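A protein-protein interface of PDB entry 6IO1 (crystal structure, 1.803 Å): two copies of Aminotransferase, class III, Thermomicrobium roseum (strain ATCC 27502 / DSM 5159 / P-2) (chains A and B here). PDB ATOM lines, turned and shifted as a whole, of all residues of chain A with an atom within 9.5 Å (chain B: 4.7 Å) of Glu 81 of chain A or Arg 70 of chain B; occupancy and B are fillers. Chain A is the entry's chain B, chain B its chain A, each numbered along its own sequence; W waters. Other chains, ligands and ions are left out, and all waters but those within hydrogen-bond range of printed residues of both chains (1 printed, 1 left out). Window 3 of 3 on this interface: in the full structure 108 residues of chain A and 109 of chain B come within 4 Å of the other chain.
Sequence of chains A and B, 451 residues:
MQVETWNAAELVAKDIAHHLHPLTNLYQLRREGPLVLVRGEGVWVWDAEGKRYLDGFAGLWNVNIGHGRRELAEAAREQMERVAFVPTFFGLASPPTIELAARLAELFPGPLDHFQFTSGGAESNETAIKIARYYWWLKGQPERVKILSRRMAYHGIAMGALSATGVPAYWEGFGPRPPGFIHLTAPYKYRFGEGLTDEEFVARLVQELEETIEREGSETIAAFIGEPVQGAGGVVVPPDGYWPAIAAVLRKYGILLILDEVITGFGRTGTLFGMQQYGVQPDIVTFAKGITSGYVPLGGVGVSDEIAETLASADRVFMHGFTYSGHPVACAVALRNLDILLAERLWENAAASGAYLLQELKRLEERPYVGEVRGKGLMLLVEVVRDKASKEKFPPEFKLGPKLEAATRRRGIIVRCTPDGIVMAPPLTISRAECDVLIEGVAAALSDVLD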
ATOM      1  N   ALA A  73      24.837 -29.089  18.453  1.00  0.00           N
ATOM      2  CA  ALA A  73      23.389 -28.916  18.491  1.00  0.00           C
ATOM      3  C   ALA A  73      22.795 -29.555  19.739  1.00  0.00           C
ATOM      4  O   ALA A  73      21.905 -28.981  20.377  1.00  0.00           O
ATOM      5  CB  ALA A  73      22.756 -29.507  17.230  1.00  0.00           C
ATOM      6  N   GLU A  74      23.271 -30.751  20.100  1.00  0.00           N
ATOM      7  CA  GLU A  74      22.770 -31.418  21.297  1.00  0.00           C
ATOM      8  C   GLU A  74      23.154 -30.659  22.558  1.00  0.00           C
ATOM      9  O   GLU A  74      22.354 -30.557  23.497  1.00  0.00           O
ATOM     10  CB  GLU A  74      23.297 -32.855  21.355  1.00  0.00           C
ATOM     11  CG  GLU A  74      23.196 -33.504  22.729  1.00  0.00           C
ATOM     12  CD  GLU A  74      21.764 -33.711  23.191  1.00  0.00           C
ATOM     13  OE1 GLU A  74      20.838 -33.618  22.357  1.00  0.00           O
ATOM     14  OE2 GLU A  74      21.562 -33.964  24.397  1.00  0.00           O
ATOM     15  N   ALA A  75      24.370 -30.113  22.598  1.00  0.00           N
ATOM     16  CA  ALA A  75      24.770 -29.301  23.743  1.00  0.00           C
ATOM     17  C   ALA A  75      23.866 -28.084  23.884  1.00  0.00           C
ATOM     18  O   ALA A  75      23.400 -27.765  24.988  1.00  0.00           O
ATOM     19  CB  ALA A  75      26.230 -28.874  23.608  1.00  0.00           C
ATOM     20  N   ALA A  76      23.597 -27.398  22.769  1.00  0.00           N
ATOM     21  CA  ALA A  76      22.715 -26.238  22.805  1.00  0.00           C
ATOM     22  C   ALA A  76      21.312 -26.620  23.257  1.00  0.00           C
ATOM     23  O   ALA A  76      20.707 -25.921  24.073  1.00  0.00           O
ATOM     24  CB  ALA A  76      22.670 -25.567  21.434  1.00  0.00           C
ATOM     25  N   ARG A  77      20.775 -27.726  22.734  1.00  0.00           N
ATOM     26  CA  ARG A  77      19.433 -28.158  23.116  1.00  0.00           C
ATOM     27  C   ARG A  77      19.360 -28.467  24.608  1.00  0.00           C
ATOM     28  O   ARG A  77      18.443 -28.016  25.308  1.00  0.00           O
ATOM     29  CB  ARG A  77      19.031 -29.381  22.290  1.00  0.00           C
ATOM     30  CG  ARG A  77      17.624 -29.889  22.550  1.00  0.00           C
ATOM     31  CD  ARG A  77      17.548 -31.400  22.376  1.00  0.00           C
ATOM     32  NE  ARG A  77      18.423 -32.109  23.307  1.00  0.00           N
ATOM     33  CZ  ARG A  77      18.128 -32.337  24.583  1.00  0.00           C
ATOM     34  NH1 ARG A  77      16.967 -31.932  25.078  1.00  0.00           N
ATOM     35  NH2 ARG A  77      18.984 -32.988  25.359  1.00  0.00           N
ATOM     36  N   GLU A  78      20.336 -29.229  25.111  1.00  0.00           N
ATOM     37  CA  GLU A  78      20.368 -29.582  26.526  1.00  0.00           C
ATOM     38  C   GLU A  78      20.427 -28.337  27.399  1.00  0.00           C
ATOM     39  O   GLU A  78      19.655 -28.194  28.358  1.00  0.00           O
ATOM     40  CB  GLU A  78      21.568 -30.490  26.797  1.00  0.00           C
ATOM     41  CG  GLU A  78      21.603 -31.120  28.178  1.00  0.00           C
ATOM     42  CD  GLU A  78      22.974 -31.669  28.521  1.00  0.00           C
ATOM     43  OE1 GLU A  78      23.464 -32.548  27.783  1.00  0.00           O
ATOM     44  OE2 GLU A  78      23.563 -31.220  29.526  1.00  0.00           O
ATOM     45  N   GLN A  79      21.345 -27.418  27.080  1.00  0.00           N
ATOM     46  CA  GLN A  79      21.479 -26.220  27.899  1.00  0.00           C
ATOM     47  C   GLN A  79      20.232 -25.351  27.820  1.00  0.00           C
ATOM     48  O   GLN A  79      19.798 -24.803  28.832  1.00  0.00           O
ATOM     49  CB  GLN A  79      22.719 -25.424  27.498  1.00  0.00           C
ATOM     50  CG  GLN A  79      23.041 -24.292  28.467  1.00  0.00           C
ATOM     51  CD  GLN A  79      23.163 -24.770  29.905  1.00  0.00           C
ATOM     52  OE1 GLN A  79      23.745 -25.822  30.175  1.00  0.00           O
ATOM     53  NE2 GLN A  79      22.606 -24.002  30.835  1.00  0.00           N
ATOM     54  N   MET A  80      19.648 -25.195  26.629  1.00  0.00           N
ATOM     55  CA  MET A  80      18.452 -24.367  26.507  1.00  0.00           C
ATOM     56  C   MET A  80      17.297 -24.940  27.315  1.00  0.00           C
ATOM     57  O   MET A  80      16.524 -24.189  27.923  1.00  0.00           O
ATOM     58  CB  MET A  80      18.061 -24.219  25.037  1.00  0.00           C
ATOM     59  CG  MET A  80      18.996 -23.324  24.255  1.00  0.00           C
ATOM     60  SD  MET A  80      18.574 -23.203  22.513  1.00  0.00           S
ATOM     61  CE  MET A  80      17.062 -22.253  22.602  1.00  0.00           C
ATOM     62  N   GLU A  81      17.155 -26.266  27.329  1.00  0.00           N
ATOM     63  CA  GLU A  81      16.103 -26.870  28.142  1.00  0.00           C
ATOM     64  C   GLU A  81      16.375 -26.696  29.633  1.00  0.00           C
ATOM     65  O   GLU A  81      15.455 -26.400  30.405  1.00  0.00           O
ATOM     66  CB  GLU A  81      15.942 -28.346  27.784  1.00  0.00           C
ATOM     67  CG  GLU A  81      15.452 -28.566  26.362  1.00  0.00           C
ATOM     68  CD  GLU A  81      14.813 -29.923  26.159  1.00  0.00           C
ATOM     69  OE1 GLU A  81      14.296 -30.492  27.143  1.00  0.00           O
ATOM     70  OE2 GLU A  81      14.831 -30.420  25.014  1.00  0.00           O
ATOM     71  N   ARG A  82      17.629 -26.870  30.061  1.00  0.00           N
ATOM     72  CA  ARG A  82      17.945 -26.735  31.482  1.00  0.00           C
ATOM     73  C   ARG A  82      17.805 -25.290  31.956  1.00  0.00           C
ATOM     74  O   ARG A  82      17.075 -25.008  32.915  1.00  0.00           O
ATOM     75  CB  ARG A  82      19.354 -27.261  31.754  1.00  0.00           C
ATOM     76  CG  ARG A  82      19.797 -27.104  33.192  1.00  0.00           C
ATOM     77  CD  ARG A  82      21.099 -27.834  33.444  1.00  0.00           C
ATOM     78  NE  ARG A  82      21.164 -29.090  32.706  1.00  0.00           N
ATOM     79  CZ  ARG A  82      22.289 -29.747  32.448  1.00  0.00           C
ATOM     80  NH1 ARG A  82      23.451 -29.263  32.863  1.00  0.00           N
ATOM     81  NH2 ARG A  82      22.255 -30.883  31.767  1.00  0.00           N
ATOM     82  N   VAL A  83      18.491 -24.364  31.289  1.00  0.00           N
ATOM     83  CA  VAL A  83      18.325 -22.925  31.470  1.00  0.00           C
ATOM     84  C   VAL A  83      19.032 -22.229  30.311  1.00  0.00           C
ATOM     85  O   VAL A  83      20.203 -22.497  30.022  1.00  0.00           O
ATOM     86  CB  VAL A  83      18.866 -22.452  32.837  1.00  0.00           C
ATOM     87  CG1 VAL A  83      20.359 -22.764  32.995  1.00  0.00           C
ATOM     88  CG2 VAL A  83      18.598 -20.971  33.030  1.00  0.00           C
ATOM     89  N   ALA A  84      18.330 -21.317  29.643  1.00  0.00           N
ATOM     90  CA  ALA A  84      18.879 -20.705  28.440  1.00  0.00           C
ATOM     91  C   ALA A  84      19.697 -19.459  28.743  1.00  0.00           C
ATOM     92  O   ALA A  84      20.741 -19.240  28.118  1.00  0.00           O
ATOM     93  CB  ALA A  84      17.758 -20.368  27.453  1.00  0.00           C
ATOM     94  N   PHE A  85      19.249 -18.628  29.681  1.00  0.00           N
ATOM     95  CA  PHE A  85      19.957 -17.394  29.987  1.00  0.00           C
ATOM     96  C   PHE A  85      20.079 -17.233  31.491  1.00  0.00           C
ATOM     97  O   PHE A  85      19.071 -17.177  32.202  1.00  0.00           O
ATOM     98  CB  PHE A  85      19.265 -16.170  29.385  1.00  0.00           C
ATOM     99  CG  PHE A  85      20.020 -14.891  29.613  1.00  0.00           C
ATOM    100  CD1 PHE A  85      21.293 -14.730  29.094  1.00  0.00           C
ATOM    101  CD2 PHE A  85      19.472 -13.864  30.363  1.00  0.00           C
ATOM    102  CE1 PHE A  85      22.002 -13.564  29.305  1.00  0.00           C
ATOM    103  CE2 PHE A  85      20.178 -12.692  30.578  1.00  0.00           C
ATOM    104  CZ  PHE A  85      21.445 -12.543  30.047  1.00  0.00           C
ATOM    105  N   PRO A 328      24.862 -18.898  28.809  1.00  0.00           N
ATOM    106  CA  PRO A 328      25.075 -20.325  29.116  1.00  0.00           C
ATOM    107  C   PRO A 328      25.060 -21.232  27.897  1.00  0.00           C
ATOM    108  O   PRO A 328      25.873 -22.162  27.816  1.00  0.00           O
ATOM    109  CB  PRO A 328      23.920 -20.646  30.076  1.00  0.00           C
ATOM    110  CG  PRO A 328      23.562 -19.330  30.686  1.00  0.00           C
ATOM    111  CD  PRO A 328      23.756 -18.322  29.592  1.00  0.00           C
ATOM    112  N   VAL A 329      24.159 -20.989  26.943  1.00  0.00           N
ATOM    113  CA  VAL A 329      24.108 -21.826  25.749  1.00  0.00           C
ATOM    114  C   VAL A 329      25.379 -21.655  24.928  1.00  0.00           C
ATOM    115  O   VAL A 329      25.966 -22.637  24.450  1.00  0.00           O
ATOM    116  CB  VAL A 329      22.851 -21.496  24.926  1.00  0.00           C
ATOM    117  CG1 VAL A 329      22.742 -22.419  23.721  1.00  0.00           C
ATOM    118  CG2 VAL A 329      21.615 -21.592  25.803  1.00  0.00           C
ATOM    119  N   GLY B  40      16.256 -23.590  35.198  1.00  0.00           N
ATOM    120  CA  GLY B  40      15.158 -22.661  35.128  1.00  0.00           C
ATOM    121  C   GLY B  40      13.890 -23.238  34.554  1.00  0.00           C
ATOM    122  O   GLY B  40      13.917 -24.069  33.645  1.00  0.00           O
ATOM    123  N   GLY B  68      12.795 -22.616  30.232  1.00  0.00           N
ATOM    124  CA  GLY B  68      12.435 -24.004  30.021  1.00  0.00           C
ATOM    125  C   GLY B  68      11.540 -24.291  28.839  1.00  0.00           C
ATOM    126  O   GLY B  68      10.867 -25.325  28.830  1.00  0.00           O
ATOM    127  N   ARG B  69      11.509 -23.418  27.835  1.00  0.00           N
ATOM    128  CA  ARG B  69      10.666 -23.640  26.666  1.00  0.00           C
ATOM    129  C   ARG B  69      11.383 -24.588  25.711  1.00  0.00           C
ATOM    130  O   ARG B  69      12.331 -24.191  25.025  1.00  0.00           O
ATOM    131  CB  ARG B  69      10.332 -22.315  25.987  1.00  0.00           C
ATOM    132  CG  ARG B  69       9.531 -21.358  26.858  1.00  0.00           C
ATOM    133  CD  ARG B  69       8.039 -21.639  26.773  1.00  0.00           C
ATOM    134  NE  ARG B  69       7.246 -20.534  27.306  1.00  0.00           N
ATOM    135  CZ  ARG B  69       5.954 -20.352  27.058  1.00  0.00           C
ATOM    136  NH1 ARG B  69       5.296 -21.205  26.285  1.00  0.00           N
ATOM    137  NH2 ARG B  69       5.316 -19.316  27.587  1.00  0.00           N
ATOM    138  N   ARG B  70      10.912 -25.831  25.662  1.00  0.00           N
ATOM    139  CA  ARG B  70      11.537 -26.859  24.794  1.00  0.00           C
ATOM    140  C   ARG B  70      11.444 -26.392  23.338  1.00  0.00           C
ATOM    141  O   ARG B  70      12.406 -26.626  22.582  1.00  0.00           O
ATOM    142  CB  ARG B  70      10.827 -28.203  24.980  1.00  0.00           C
ATOM    143  CG  ARG B  70      11.051 -28.841  26.344  1.00  0.00           C
ATOM    144  CD  ARG B  70      10.465 -30.237  26.433  1.00  0.00           C
ATOM    145  NE  ARG B  70      10.782 -30.891  27.695  1.00  0.00           N
ATOM    146  CZ  ARG B  70      10.431 -32.132  28.010  1.00  0.00           C
ATOM    147  NH1 ARG B  70       9.743 -32.863  27.148  1.00  0.00           N
ATOM    148  NH2 ARG B  70      10.767 -32.638  29.182  1.00  0.00           N
ATOM    149  N   GLU B  71      10.345 -25.720  22.980  1.00  0.00           N
ATOM    150  CA  GLU B  71      10.128 -25.349  21.586  1.00  0.00           C
ATOM    151  C   GLU B  71      11.329 -24.592  21.027  1.00  0.00           C
ATOM    152  O   GLU B  71      11.802 -24.883  19.920  1.00  0.00           O
ATOM    153  CB  GLU B  71       8.858 -24.504  21.468  1.00  0.00           C
ATOM    154  CG  GLU B  71       7.594 -25.184  21.990  1.00  0.00           C
ATOM    155  CD  GLU B  71       7.258 -24.799  23.422  1.00  0.00           C
ATOM    156  OE1 GLU B  71       8.193 -24.617  24.230  1.00  0.00           O
ATOM    157  OE2 GLU B  71       6.056 -24.679  23.741  1.00  0.00           O
ATOM    158  N   LEU B  72      11.855 -23.636  21.796  1.00  0.00           N
ATOM    159  CA  LEU B  72      13.010 -22.867  21.343  1.00  0.00           C
ATOM    160  C   LEU B  72      14.258 -23.737  21.268  1.00  0.00           C
ATOM    161  O   LEU B  72      15.074 -23.589  20.347  1.00  0.00           O
ATOM    162  CB  LEU B  72      13.233 -21.666  22.265  1.00  0.00           C
ATOM    163  CG  LEU B  72      12.467 -20.378  21.932  1.00  0.00           C
ATOM    164  CD1 LEU B  72      10.965 -20.614  21.832  1.00  0.00           C
ATOM    165  CD2 LEU B  72      12.759 -19.289  22.950  1.00  0.00           C
ATOM    166  N   ALA B  73      14.428 -24.647  22.232  1.00  0.00           N
ATOM    167  CA  ALA B  73      15.564 -25.561  22.193  1.00  0.00           C
ATOM    168  C   ALA B  73      15.526 -26.434  20.947  1.00  0.00           C
ATOM    169  O   ALA B  73      16.552 -26.631  20.286  1.00  0.00           O
ATOM    170  CB  ALA B  73      15.587 -26.423  23.454  1.00  0.00           C
ATOM    171  N   GLU B  74      14.344 -26.953  20.602  1.00  0.00           N
ATOM    172  CA  GLU B  74      14.218 -27.782  19.409  1.00  0.00           C
ATOM    173  C   GLU B  74      14.449 -26.961  18.145  1.00  0.00           C
ATOM    174  O   GLU B  74      15.041 -27.452  17.179  1.00  0.00           O
ATOM    175  CB  GLU B  74      12.850 -28.458  19.372  1.00  0.00           C
ATOM    176  CG  GLU B  74      12.450 -29.001  18.005  1.00  0.00           C
ATOM    177  CD  GLU B  74      13.028 -30.380  17.730  1.00  0.00           C
ATOM    178  OE1 GLU B  74      12.752 -30.950  16.652  1.00  0.00           O
ATOM    179  OE2 GLU B  74      13.767 -30.896  18.594  1.00  0.00           O
HETATM  180  O   HOH W   1      15.563 -21.921  29.354  1.00  0.00           O
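The guanidinium group (NE) of Arg 70 of chain B is in salt-bridge range of the side-chain carboxylate (OE1) of Glu 81 of chain A, at 3.6 Å.
N of Gly 40 of chain B lies within hydrogen-bond range of O of Arg 82 of chain A (2.8 Å).
The guanidinium group (NH1) of Arg 77 of chain A lies within salt-bridge range of the side-chain carboxylate (OE2) of Glu 81 of chain A (2.6 Å).
The side-chain carboxylate (OE2) of Glu 78 of chain A lies within salt-bridge range of the guanidinium group (NH2) of Arg 82 of chain A (2.6 Å).
The side-chain amide nitrogen (NE2) of Gln 79 of chain A lies within hydrogen-bond range of the backbone carbonyl oxygen (O) of Val 83 of chain A (2.9 Å).
NH2 of Arg 77 of chain A is in salt-bridge range of OE2 of Glu 74 of chain A (2.9 Å).
Arg 77 of chain A touches Ala 73 of chain B (O to CB, 3.8 Å).
Leu 72 of chain B touches Met 80 of chain A.
Ala 73 of chain B touches Met 80 of chain A.
Gly 68 of chain B touches Glu 81 of chain A (CA to O, 3.9 Å).
CB of Ala 73 of chain B touches CG of Glu 81 of chain A, 3.6 Å away.
CB of Val 83 of chain A touches N of Gly 40 of chain B, 3.7 Å away.
Glu 81 of chain A touches just these residues of chain B: Gly 68 (3.9 Å), Arg 70 (3.6 Å) and Ala 73 (3.6 Å).
Of chain A, only Glu 81 comes within 4 Å of Arg 70 of chain B.
Of chain A, only Glu 81 comes within 4 Å of Gly 68 of chain B.
No residue of chain A comes within 4 Å of Glu 71 of chain B.
Ala 73 of chain B touches just these residues of chain A: Arg 77, Met 80 and Glu 81.
Of the printed residues of chain B, Arg 82 of chain A touches Gly 40 (2.8 Å).
Printed residues of chain B within 4 Å of Met 80 of chain A: Leu 72 (3.3 Å) and Ala 73 (3.6 Å).
Printed residues of chain B within 4 Å of Arg 77 of chain A: Ala 73.
Of the printed residues of chain A, Gly 40 of chain B touches Arg 82 and Val 83.
Val 329 of chain A touches none of the printed residues of chain B.
Ala 76 of chain A touches none of the printed residues of chain B.
The nearest printed residue of chain B that does not touch Val 83 of chain A is Gly 68 of chain B (5.7 Å).
Hydrophobic or aromatic side chains of chain B that line the printed part of chain A: Leu 72 and Ala 73.
Among the printed residues, 8 pairs touch across the chains.
2 positions are printed for both chains.
Of the 8 pairs that touch across the chains among the printed residues, none has its exchanged pair printed and touching as well.
Water W1 lies within hydrogen-bond range of the backbone NH of Ala 84 of chain A (2.8 Å), the backbone carbonyl oxygen of Met 80 of chain A (2.8 Å) and the backbone NH of Gly 68 of chain B (3.0 Å).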
